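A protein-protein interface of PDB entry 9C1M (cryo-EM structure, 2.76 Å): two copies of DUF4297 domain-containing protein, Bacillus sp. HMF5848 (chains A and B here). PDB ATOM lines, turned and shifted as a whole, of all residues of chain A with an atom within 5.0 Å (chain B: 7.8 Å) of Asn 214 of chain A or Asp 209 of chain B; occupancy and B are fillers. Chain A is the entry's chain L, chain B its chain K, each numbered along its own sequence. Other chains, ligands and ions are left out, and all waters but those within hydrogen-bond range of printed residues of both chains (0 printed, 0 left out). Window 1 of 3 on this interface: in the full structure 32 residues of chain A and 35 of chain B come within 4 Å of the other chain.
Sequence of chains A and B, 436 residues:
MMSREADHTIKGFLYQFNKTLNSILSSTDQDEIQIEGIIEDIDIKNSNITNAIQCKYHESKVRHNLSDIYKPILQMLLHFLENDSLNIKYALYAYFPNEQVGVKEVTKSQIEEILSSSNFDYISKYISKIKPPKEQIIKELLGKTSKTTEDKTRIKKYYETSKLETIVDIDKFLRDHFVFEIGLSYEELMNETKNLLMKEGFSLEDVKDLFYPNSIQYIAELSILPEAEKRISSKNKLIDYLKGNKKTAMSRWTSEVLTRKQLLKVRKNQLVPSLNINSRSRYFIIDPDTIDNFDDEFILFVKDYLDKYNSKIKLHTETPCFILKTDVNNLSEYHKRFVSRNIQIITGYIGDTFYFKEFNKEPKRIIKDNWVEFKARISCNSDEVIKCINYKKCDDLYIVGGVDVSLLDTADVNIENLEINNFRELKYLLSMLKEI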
ATOM      1  N   LEU A 210     -19.524 -32.722  -0.291  1.00  0.00           N
ATOM      2  CA  LEU A 210     -18.996 -31.370  -0.158  1.00  0.00           C
ATOM      3  C   LEU A 210     -20.027 -30.367   0.334  1.00  0.00           C
ATOM      4  O   LEU A 210     -19.764 -29.643   1.302  1.00  0.00           O
ATOM      5  CB  LEU A 210     -18.426 -30.904  -1.509  1.00  0.00           C
ATOM      6  CG  LEU A 210     -17.761 -29.528  -1.565  1.00  0.00           C
ATOM      7  CD1 LEU A 210     -16.324 -29.592  -1.075  1.00  0.00           C
ATOM      8  CD2 LEU A 210     -17.824 -28.958  -2.974  1.00  0.00           C
ATOM      9  N   PHE A 211     -21.198 -30.302  -0.304  1.00  0.00           N
ATOM     10  CA  PHE A 211     -22.112 -29.187  -0.072  1.00  0.00           C
ATOM     11  C   PHE A 211     -22.708 -29.221   1.331  1.00  0.00           C
ATOM     12  O   PHE A 211     -22.715 -28.204   2.033  1.00  0.00           O
ATOM     13  CB  PHE A 211     -23.215 -29.192  -1.129  1.00  0.00           C
ATOM     14  CG  PHE A 211     -22.747 -28.751  -2.486  1.00  0.00           C
ATOM     15  CD1 PHE A 211     -22.117 -27.530  -2.650  1.00  0.00           C
ATOM     16  CD2 PHE A 211     -22.927 -29.562  -3.594  1.00  0.00           C
ATOM     17  CE1 PHE A 211     -21.681 -27.120  -3.894  1.00  0.00           C
ATOM     18  CE2 PHE A 211     -22.491 -29.157  -4.842  1.00  0.00           C
ATOM     19  CZ  PHE A 211     -21.869 -27.934  -4.991  1.00  0.00           C
ATOM     20  N   TYR A 212     -23.229 -30.373   1.755  1.00  0.00           N
ATOM     21  CA  TYR A 212     -23.861 -30.447   3.071  1.00  0.00           C
ATOM     22  C   TYR A 212     -22.880 -30.214   4.215  1.00  0.00           C
ATOM     23  O   TYR A 212     -23.199 -29.414   5.114  1.00  0.00           O
ATOM     24  CB  TYR A 212     -24.598 -31.784   3.218  1.00  0.00           C
ATOM     25  CG  TYR A 212     -25.258 -31.980   4.564  1.00  0.00           C
ATOM     26  CD1 TYR A 212     -26.451 -31.338   4.872  1.00  0.00           C
ATOM     27  CD2 TYR A 212     -24.693 -32.808   5.524  1.00  0.00           C
ATOM     28  CE1 TYR A 212     -27.060 -31.513   6.100  1.00  0.00           C
ATOM     29  CE2 TYR A 212     -25.295 -32.990   6.755  1.00  0.00           C
ATOM     30  CZ  TYR A 212     -26.478 -32.341   7.038  1.00  0.00           C
ATOM     31  OH  TYR A 212     -27.082 -32.519   8.261  1.00  0.00           O
ATOM     32  N   PRO A 213     -21.713 -30.873   4.277  1.00  0.00           N
ATOM     33  CA  PRO A 213     -20.772 -30.552   5.364  1.00  0.00           C
ATOM     34  C   PRO A 213     -20.294 -29.111   5.343  1.00  0.00           C
ATOM     35  O   PRO A 213     -20.137 -28.500   6.408  1.00  0.00           O
ATOM     36  CB  PRO A 213     -19.619 -31.540   5.133  1.00  0.00           C
ATOM     37  CG  PRO A 213     -20.223 -32.648   4.345  1.00  0.00           C
ATOM     38  CD  PRO A 213     -21.211 -31.983   3.446  1.00  0.00           C
ATOM     39  N   ASN A 214     -20.068 -28.545   4.154  1.00  0.00           N
ATOM     40  CA  ASN A 214     -19.650 -27.149   4.072  1.00  0.00           C
ATOM     41  C   ASN A 214     -20.735 -26.218   4.593  1.00  0.00           C
ATOM     42  O   ASN A 214     -20.446 -25.259   5.315  1.00  0.00           O
ATOM     43  CB  ASN A 214     -19.286 -26.787   2.633  1.00  0.00           C
ATOM     44  CG  ASN A 214     -17.831 -27.057   2.317  1.00  0.00           C
ATOM     45  OD1 ASN A 214     -16.968 -26.957   3.187  1.00  0.00           O
ATOM     46  ND2 ASN A 214     -17.550 -27.394   1.064  1.00  0.00           N
ATOM     47  N   SER A 215     -21.992 -26.487   4.238  1.00  0.00           N
ATOM     48  CA  SER A 215     -23.092 -25.665   4.728  1.00  0.00           C
ATOM     49  C   SER A 215     -23.243 -25.788   6.240  1.00  0.00           C
ATOM     50  O   SER A 215     -23.490 -24.790   6.926  1.00  0.00           O
ATOM     51  CB  SER A 215     -24.389 -26.051   4.019  1.00  0.00           C
ATOM     52  OG  SER A 215     -24.276 -25.873   2.619  1.00  0.00           O
ATOM     53  N   ILE A 216     -23.099 -27.003   6.777  1.00  0.00           N
ATOM     54  CA  ILE A 216     -23.191 -27.187   8.223  1.00  0.00           C
ATOM     55  C   ILE A 216     -22.072 -26.431   8.929  1.00  0.00           C
ATOM     56  O   ILE A 216     -22.295 -25.774   9.955  1.00  0.00           O
ATOM     57  CB  ILE A 216     -23.178 -28.686   8.577  1.00  0.00           C
ATOM     58  CG1 ILE A 216     -24.442 -29.369   8.051  1.00  0.00           C
ATOM     59  CG2 ILE A 216     -23.060 -28.880  10.081  1.00  0.00           C
ATOM     60  CD1 ILE A 216     -25.723 -28.827   8.645  1.00  0.00           C
ATOM     61  N   GLN A 217     -20.851 -26.510   8.392  1.00  0.00           N
ATOM     62  CA  GLN A 217     -19.734 -25.775   8.976  1.00  0.00           C
ATOM     63  C   GLN A 217     -19.963 -24.271   8.900  1.00  0.00           C
ATOM     64  O   GLN A 217     -19.627 -23.538   9.835  1.00  0.00           O
ATOM     65  CB  GLN A 217     -18.431 -26.156   8.272  1.00  0.00           C
ATOM     66  CG  GLN A 217     -17.194 -25.470   8.833  1.00  0.00           C
ATOM     67  CD  GLN A 217     -16.888 -25.890  10.257  1.00  0.00           C
ATOM     68  OE1 GLN A 217     -17.231 -26.994  10.680  1.00  0.00           O
ATOM     69  NE2 GLN A 217     -16.236 -25.008  11.006  1.00  0.00           N
ATOM     70  N   TYR A 218     -20.527 -23.793   7.788  1.00  0.00           N
ATOM     71  CA  TYR A 218     -20.823 -22.371   7.649  1.00  0.00           C
ATOM     72  C   TYR A 218     -21.850 -21.917   8.680  1.00  0.00           C
ATOM     73  O   TYR A 218     -21.694 -20.858   9.302  1.00  0.00           O
ATOM     74  CB  TYR A 218     -21.312 -22.093   6.226  1.00  0.00           C
ATOM     75  CG  TYR A 218     -21.720 -20.666   5.949  1.00  0.00           C
ATOM     76  CD1 TYR A 218     -20.765 -19.678   5.742  1.00  0.00           C
ATOM     77  CD2 TYR A 218     -23.060 -20.309   5.869  1.00  0.00           C
ATOM     78  CE1 TYR A 218     -21.134 -18.373   5.478  1.00  0.00           C
ATOM     79  CE2 TYR A 218     -23.438 -19.007   5.604  1.00  0.00           C
ATOM     80  CZ  TYR A 218     -22.470 -18.043   5.409  1.00  0.00           C
ATOM     81  OH  TYR A 218     -22.843 -16.745   5.148  1.00  0.00           O
ATOM     82  N   TYR A 241     -21.119 -19.121  -2.113  1.00  0.00           N
ATOM     83  CA  TYR A 241     -19.991 -19.679  -1.372  1.00  0.00           C
ATOM     84  C   TYR A 241     -19.762 -21.141  -1.740  1.00  0.00           C
ATOM     85  O   TYR A 241     -18.623 -21.566  -1.978  1.00  0.00           O
ATOM     86  CB  TYR A 241     -20.240 -19.520   0.129  1.00  0.00           C
ATOM     87  CG  TYR A 241     -19.294 -20.289   1.024  1.00  0.00           C
ATOM     88  CD1 TYR A 241     -18.002 -19.834   1.255  1.00  0.00           C
ATOM     89  CD2 TYR A 241     -19.700 -21.457   1.656  1.00  0.00           C
ATOM     90  CE1 TYR A 241     -17.137 -20.529   2.079  1.00  0.00           C
ATOM     91  CE2 TYR A 241     -18.842 -22.159   2.482  1.00  0.00           C
ATOM     92  CZ  TYR A 241     -17.563 -21.689   2.691  1.00  0.00           C
ATOM     93  OH  TYR A 241     -16.705 -22.386   3.513  1.00  0.00           O
ATOM     94  N   LEU A 242     -20.843 -21.924  -1.808  1.00  0.00           N
ATOM     95  CA  LEU A 242     -20.718 -23.330  -2.181  1.00  0.00           C
ATOM     96  C   LEU A 242     -20.201 -23.482  -3.606  1.00  0.00           C
ATOM     97  O   LEU A 242     -19.345 -24.334  -3.876  1.00  0.00           O
ATOM     98  CB  LEU A 242     -22.063 -24.038  -2.019  1.00  0.00           C
ATOM     99  CG  LEU A 242     -22.574 -24.214  -0.587  1.00  0.00           C
ATOM    100  CD1 LEU A 242     -23.961 -24.840  -0.586  1.00  0.00           C
ATOM    101  CD2 LEU A 242     -21.604 -25.052   0.230  1.00  0.00           C
ATOM    102  N   ASN A 245     -16.472 -22.656  -3.667  1.00  0.00           N
ATOM    103  CA  ASN A 245     -15.696 -23.760  -3.109  1.00  0.00           C
ATOM    104  C   ASN A 245     -15.606 -24.919  -4.093  1.00  0.00           C
ATOM    105  O   ASN A 245     -14.531 -25.505  -4.278  1.00  0.00           O
ATOM    106  CB  ASN A 245     -16.311 -24.228  -1.791  1.00  0.00           C
ATOM    107  CG  ASN A 245     -16.048 -23.268  -0.651  1.00  0.00           C
ATOM    108  OD1 ASN A 245     -15.381 -22.247  -0.823  1.00  0.00           O
ATOM    109  ND2 ASN A 245     -16.563 -23.597   0.526  1.00  0.00           N
ATOM    110  N   THR A 248     -13.207 -23.948  -6.967  1.00  0.00           N
ATOM    111  CA  THR A 248     -11.816 -23.967  -6.527  1.00  0.00           C
ATOM    112  C   THR A 248     -11.311 -25.395  -6.364  1.00  0.00           C
ATOM    113  O   THR A 248     -10.197 -25.720  -6.793  1.00  0.00           O
ATOM    114  CB  THR A 248     -11.667 -23.193  -5.217  1.00  0.00           C
ATOM    115  OG1 THR A 248     -12.261 -21.896  -5.356  1.00  0.00           O
ATOM    116  CG2 THR A 248     -10.197 -23.035  -4.856  1.00  0.00           C
ATOM    117  N   ALA A 249     -12.122 -26.265  -5.755  1.00  0.00           N
ATOM    118  CA  ALA A 249     -11.725 -27.660  -5.602  1.00  0.00           C
ATOM    119  C   ALA A 249     -11.569 -28.341  -6.956  1.00  0.00           C
ATOM    120  O   ALA A 249     -10.624 -29.111  -7.165  1.00  0.00           O
ATOM    121  CB  ALA A 249     -12.743 -28.405  -4.738  1.00  0.00           C
ATOM    122  N   ARG A 252      -8.304 -27.078  -8.549  1.00  0.00           N
ATOM    123  CA  ARG A 252      -7.131 -27.574  -7.837  1.00  0.00           C
ATOM    124  C   ARG A 252      -6.906 -29.057  -8.097  1.00  0.00           C
ATOM    125  O   ARG A 252      -5.765 -29.495  -8.283  1.00  0.00           O
ATOM    126  CB  ARG A 252      -7.284 -27.303  -6.341  1.00  0.00           C
ATOM    127  CG  ARG A 252      -6.079 -27.686  -5.501  1.00  0.00           C
ATOM    128  CD  ARG A 252      -6.234 -27.187  -4.072  1.00  0.00           C
ATOM    129  NE  ARG A 252      -7.385 -27.780  -3.404  1.00  0.00           N
ATOM    130  CZ  ARG A 252      -8.533 -27.152  -3.185  1.00  0.00           C
ATOM    131  NH1 ARG A 252      -8.721 -25.901  -3.574  1.00  0.00           N
ATOM    132  NH2 ARG A 252      -9.517 -27.795  -2.564  1.00  0.00           N
ATOM    133  N   LYS B 194      -5.678 -27.951  11.593  1.00  0.00           N
ATOM    134  CA  LYS B 194      -5.416 -27.830  10.162  1.00  0.00           C
ATOM    135  C   LYS B 194      -3.957 -28.139   9.840  1.00  0.00           C
ATOM    136  O   LYS B 194      -3.660 -28.771   8.819  1.00  0.00           O
ATOM    137  CB  LYS B 194      -5.796 -26.433   9.674  1.00  0.00           C
ATOM    138  CG  LYS B 194      -7.296 -26.205   9.576  1.00  0.00           C
ATOM    139  CD  LYS B 194      -7.625 -24.750   9.294  1.00  0.00           C
ATOM    140  CE  LYS B 194      -9.127 -24.534   9.208  1.00  0.00           C
ATOM    141  NZ  LYS B 194      -9.483 -23.089   9.154  1.00  0.00           N
ATOM    142  N   SER B 203      -3.477 -30.797   1.143  1.00  0.00           N
ATOM    143  CA  SER B 203      -3.085 -29.414   0.917  1.00  0.00           C
ATOM    144  C   SER B 203      -3.951 -28.464   1.739  1.00  0.00           C
ATOM    145  O   SER B 203      -5.061 -28.796   2.165  1.00  0.00           O
ATOM    146  CB  SER B 203      -3.180 -29.064  -0.569  1.00  0.00           C
ATOM    147  OG  SER B 203      -4.516 -28.783  -0.945  1.00  0.00           O
ATOM    148  N   LEU B 204      -3.419 -27.258   1.961  1.00  0.00           N
ATOM    149  CA  LEU B 204      -4.103 -26.283   2.806  1.00  0.00           C
ATOM    150  C   LEU B 204      -5.464 -25.905   2.236  1.00  0.00           C
ATOM    151  O   LEU B 204      -6.453 -25.826   2.974  1.00  0.00           O
ATOM    152  CB  LEU B 204      -3.230 -25.040   2.981  1.00  0.00           C
ATOM    153  CG  LEU B 204      -3.823 -23.904   3.817  1.00  0.00           C
ATOM    154  CD1 LEU B 204      -4.116 -24.376   5.232  1.00  0.00           C
ATOM    155  CD2 LEU B 204      -2.892 -22.702   3.828  1.00  0.00           C
ATOM    156  N   GLU B 205      -5.535 -25.663   0.925  1.00  0.00           N
ATOM    157  CA  GLU B 205      -6.819 -25.358   0.302  1.00  0.00           C
ATOM    158  C   GLU B 205      -7.769 -26.545   0.395  1.00  0.00           C
ATOM    159  O   GLU B 205      -8.965 -26.375   0.664  1.00  0.00           O
ATOM    160  CB  GLU B 205      -6.612 -24.948  -1.156  1.00  0.00           C
ATOM    161  CG  GLU B 205      -5.997 -23.568  -1.332  1.00  0.00           C
ATOM    162  CD  GLU B 205      -6.957 -22.453  -0.968  1.00  0.00           C
ATOM    163  OE1 GLU B 205      -8.178 -22.629  -1.164  1.00  0.00           O
ATOM    164  OE2 GLU B 205      -6.490 -21.399  -0.485  1.00  0.00           O
ATOM    165  N   ASP B 206      -7.253 -27.758   0.175  1.00  0.00           N
ATOM    166  CA  ASP B 206      -8.082 -28.952   0.299  1.00  0.00           C
ATOM    167  C   ASP B 206      -8.596 -29.119   1.722  1.00  0.00           C
ATOM    168  O   ASP B 206      -9.765 -29.462   1.930  1.00  0.00           O
ATOM    169  CB  ASP B 206      -7.292 -30.188  -0.132  1.00  0.00           C
ATOM    170  CG  ASP B 206      -7.223 -30.340  -1.637  1.00  0.00           C
ATOM    171  OD1 ASP B 206      -8.258 -30.131  -2.305  1.00  0.00           O
ATOM    172  OD2 ASP B 206      -6.135 -30.671  -2.153  1.00  0.00           O
ATOM    173  N   VAL B 207      -7.738 -28.880   2.715  1.00  0.00           N
ATOM    174  CA  VAL B 207      -8.164 -28.979   4.109  1.00  0.00           C
ATOM    175  C   VAL B 207      -9.242 -27.945   4.408  1.00  0.00           C
ATOM    176  O   VAL B 207     -10.265 -28.248   5.034  1.00  0.00           O
ATOM    177  CB  VAL B 207      -6.956 -28.826   5.052  1.00  0.00           C
ATOM    178  CG1 VAL B 207      -7.421 -28.618   6.485  1.00  0.00           C
ATOM    179  CG2 VAL B 207      -6.053 -30.043   4.952  1.00  0.00           C
ATOM    180  N   LYS B 208      -9.034 -26.709   3.951  1.00  0.00           N
ATOM    181  CA  LYS B 208      -9.980 -25.637   4.242  1.00  0.00           C
ATOM    182  C   LYS B 208     -11.336 -25.890   3.592  1.00  0.00           C
ATOM    183  O   LYS B 208     -12.379 -25.636   4.205  1.00  0.00           O
ATOM    184  CB  LYS B 208      -9.409 -24.296   3.784  1.00  0.00           C
ATOM    185  CG  LYS B 208      -8.359 -23.717   4.719  1.00  0.00           C
ATOM    186  CD  LYS B 208      -7.828 -22.390   4.199  1.00  0.00           C
ATOM    187  CE  LYS B 208      -6.859 -21.760   5.185  1.00  0.00           C
ATOM    188  NZ  LYS B 208      -6.279 -20.492   4.660  1.00  0.00           N
ATOM    189  N   ASP B 209     -11.345 -26.388   2.355  1.00  0.00           N
ATOM    190  CA  ASP B 209     -12.597 -26.519   1.617  1.00  0.00           C
ATOM    191  C   ASP B 209     -13.320 -27.833   1.887  1.00  0.00           C
ATOM    192  O   ASP B 209     -14.541 -27.835   2.075  1.00  0.00           O
ATOM    193  CB  ASP B 209     -12.335 -26.374   0.115  1.00  0.00           C
ATOM    194  CG  ASP B 209     -11.803 -25.003  -0.252  1.00  0.00           C
ATOM    195  OD1 ASP B 209     -11.956 -24.067   0.560  1.00  0.00           O
ATOM    196  OD2 ASP B 209     -11.233 -24.860  -1.355  1.00  0.00           O
ATOM    197  N   LEU B 210     -12.602 -28.954   1.909  1.00  0.00           N
ATOM    198  CA  LEU B 210     -13.208 -30.277   1.997  1.00  0.00           C
ATOM    199  C   LEU B 210     -12.872 -31.014   3.284  1.00  0.00           C
ATOM    200  O   LEU B 210     -13.778 -31.470   3.988  1.00  0.00           O
ATOM    201  CB  LEU B 210     -12.768 -31.127   0.795  1.00  0.00           C
ATOM    202  CG  LEU B 210     -13.318 -32.554   0.718  1.00  0.00           C
ATOM    203  CD1 LEU B 210     -14.667 -32.588   0.017  1.00  0.00           C
ATOM    204  CD2 LEU B 210     -12.326 -33.481   0.033  1.00  0.00           C
ATOM    205  N   PHE B 211     -11.584 -31.146   3.607  1.00  0.00           N
ATOM    206  CA  PHE B 211     -11.167 -32.102   4.629  1.00  0.00           C
ATOM    207  C   PHE B 211     -11.625 -31.682   6.022  1.00  0.00           C
ATOM    208  O   PHE B 211     -12.184 -32.492   6.768  1.00  0.00           O
ATOM    209  CB  PHE B 211      -9.649 -32.277   4.583  1.00  0.00           C
ATOM    210  CG  PHE B 211      -9.174 -33.077   3.405  1.00  0.00           C
ATOM    211  CD1 PHE B 211      -9.611 -34.376   3.214  1.00  0.00           C
ATOM    212  CD2 PHE B 211      -8.303 -32.527   2.480  1.00  0.00           C
ATOM    213  CE1 PHE B 211      -9.181 -35.116   2.129  1.00  0.00           C
ATOM    214  CE2 PHE B 211      -7.870 -33.263   1.392  1.00  0.00           C
ATOM    215  CZ  PHE B 211      -8.310 -34.559   1.218  1.00  0.00           C
ATOM    216  N   TYR B 212     -11.387 -30.425   6.398  1.00  0.00           N
ATOM    217  CA  TYR B 212     -11.789 -29.978   7.732  1.00  0.00           C
ATOM    218  C   TYR B 212     -13.300 -29.986   7.932  1.00  0.00           C
ATOM    219  O   TYR B 212     -13.756 -30.481   8.979  1.00  0.00           O
ATOM    220  CB  TYR B 212     -11.193 -28.598   8.028  1.00  0.00           C
ATOM    221  CG  TYR B 212     -11.650 -28.022   9.350  1.00  0.00           C
ATOM    222  CD1 TYR B 212     -11.129 -28.494  10.548  1.00  0.00           C
ATOM    223  CD2 TYR B 212     -12.607 -27.017   9.402  1.00  0.00           C
ATOM    224  CE1 TYR B 212     -11.544 -27.978  11.760  1.00  0.00           C
ATOM    225  CE2 TYR B 212     -13.029 -26.494  10.611  1.00  0.00           C
ATOM    226  CZ  TYR B 212     -12.493 -26.979  11.786  1.00  0.00           C
ATOM    227  OH  TYR B 212     -12.907 -26.466  12.993  1.00  0.00           O
ATOM    228  N   PRO B 213     -14.125 -29.437   7.027  1.00  0.00           N
ATOM    229  CA  PRO B 213     -15.581 -29.546   7.236  1.00  0.00           C
ATOM    230  C   PRO B 213     -16.076 -30.980   7.272  1.00  0.00           C
ATOM    231  O   PRO B 213     -16.972 -31.302   8.064  1.00  0.00           O
ATOM    232  CB  PRO B 213     -16.163 -28.768   6.047  1.00  0.00           C
ATOM    233  CG  PRO B 213     -15.075 -27.846   5.629  1.00  0.00           C
ATOM    234  CD  PRO B 213     -13.815 -28.621   5.839  1.00  0.00           C
ATOM    235  N   ASN B 214     -15.509 -31.859   6.440  1.00  0.00           N
ATOM    236  CA  ASN B 214     -15.905 -33.263   6.470  1.00  0.00           C
ATOM    237  C   ASN B 214     -15.542 -33.907   7.800  1.00  0.00           C
ATOM    238  O   ASN B 214     -16.331 -34.677   8.360  1.00  0.00           O
ATOM    239  CB  ASN B 214     -15.254 -34.022   5.315  1.00  0.00           C
ATOM    240  CG  ASN B 214     -16.083 -33.980   4.049  1.00  0.00           C
ATOM    241  OD1 ASN B 214     -17.310 -33.926   4.100  1.00  0.00           O
ATOM    242  ND2 ASN B 214     -15.414 -34.011   2.904  1.00  0.00           N
ATOM    243  N   GLN B 217     -17.987 -32.632  10.434  1.00  0.00           N
ATOM    244  CA  GLN B 217     -19.277 -33.298  10.279  1.00  0.00           C
ATOM    245  C   GLN B 217     -19.216 -34.737  10.777  1.00  0.00           C
ATOM    246  O   GLN B 217     -20.160 -35.222  11.409  1.00  0.00           O
ATOM    247  CB  GLN B 217     -19.720 -33.252   8.816  1.00  0.00           C
ATOM    248  CG  GLN B 217     -21.076 -33.888   8.555  1.00  0.00           C
ATOM    249  CD  GLN B 217     -22.211 -33.151   9.238  1.00  0.00           C
ATOM    250  OE1 GLN B 217     -22.125 -31.949   9.489  1.00  0.00           O
ATOM    251  NE2 GLN B 217     -23.284 -33.871   9.545  1.00  0.00           N
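Of the 14 printed residues of chain B, 9 touch a printed residue of chain A.
Hydrophobic or aromatic side chains of chain B that line the printed part of chain A: Leu 210, Tyr 212 and Pro 213.
Of the 15 printed residues of chain A, 7 touch a printed residue of chain B.
Printed residues of chain A that touch a printed residue of chain B: Leu 210, Tyr 212, Pro 213, Asn 214, Ile 216, Gln 217 and Arg 252.
Hydrophobic or aromatic side chains of chain A within 4 Å of the printed part of chain B: Leu 210, Tyr 212, Pro 213 and Ile 216.
Among the printed residues, Asp or Glu carboxylates within 4 Å of a Lys or Arg side-chain nitrogen of the other chain: Arg 252 of chain A with Asp 206 of chain B and Arg 252 of chain A with Asp 209 of chain B.
Among the printed residues, merely in contact across the chains: Pro 213 of chain A with Asn 214 of chain B (3.2 Å), Asn 214 of chain A with Pro 213 of chain B (3.2 Å), Ile 216 of chain A with Gln 217 of chain B (3.3 Å), Arg 252 of chain A with Glu 205 of chain B (3.3 Å), Tyr 212 of chain A with Gln 217 of chain B (3.6 Å), Gln 217 of chain A with Tyr 212 of chain B (3.6 Å), Leu 210 of chain A with Leu 210 of chain B (3.6 Å), Arg 252 of chain A with Ser 203 of chain B (3.9 Å) and Pro 213 of chain A with Pro 213 of chain B (3.96 Å).
Leu 210 of chain B touches its own counterpart, Leu 210 of chain A.
Tyr 212 of chain A touches Gln 217 of chain B, and with the chains exchanged Gln 217 of chain A touches Tyr 212 of chain B.
Pro 213 of chain B touches its own counterpart, Pro 213 of chain A.
Pro 213 of chain A touches Asn 214 of chain B, and with the chains exchanged Asn 214 of chain A touches Pro 213 of chain B.
Positions printed for both chains: 210, 211, 212, 213, 214 and 217.
The backbone carbonyl oxygen (O) of Val 207 of chain B sits at hydrogen-bond distance from the backbone NH (N) of Tyr 212 of chain B (2.8 Å).
OD2 of Asp 206 of chain B sits at hydrogen-bond distance from OG of Ser 203 of chain B.
N of Phe 211 of chain B is in hydrogen-bond range of O of Asp 206 of chain B, 3.0 Å away.
The side-chain amide nitrogen of Asn 214 of chain A lies within hydrogen-bond range of the backbone carbonyl oxygen of Leu 210 of chain A, at 3.2 Å.
The side-chain amide nitrogen of Asn 214 of chain B is in hydrogen-bond range of the backbone carbonyl oxygen of Leu 210 of chain B (3.2 Å).
Of chain B, only Asp 209 (2.8 Å) and Pro 213 (3.2 Å) come within 4 Å of Asn 214 of chain A.
Asp 209 of chain B touches just these residues of chain A: Asn 214 (2.8 Å) and Arg 252 (3.5 Å).
Printed residues of chain A within 4 Å of Gln 217 of chain B: Tyr 212 (3.6 Å) and Ile 216 (3.3 Å).
Of the printed residues of chain A, Asp 206 of chain B touches Arg 252.
Ser 215 of chain A touches none of the printed residues of chain B.
The nearest residue of chain B that does not touch Asn 214 of chain A is Lys 208 of chain B (4.9 Å).
The nearest residue of chain A that does not touch Asp 209 of chain B is Leu 210 of chain A (4.02 Å).
The nearest printed residue of chain A that does not touch Gln 217 of chain B is Pro 213 of chain A (4.1 Å).
The side-chain carboxylate (OD1) of Asp 206 of chain B lies within salt-bridge range of the guanidinium group (NH2) of Arg 252 of chain A, 2.7 Å away.
The guanidinium group (NH1) of Arg 252 of chain A is in salt-bridge range of the side-chain carboxylate (OD2) of Asp 209 of chain B (3.5 Å).
The side-chain amide oxygen of Asn 214 of chain A lies close to the backbone carbonyl oxygen of Asp 209 of chain B (2.8 Å).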
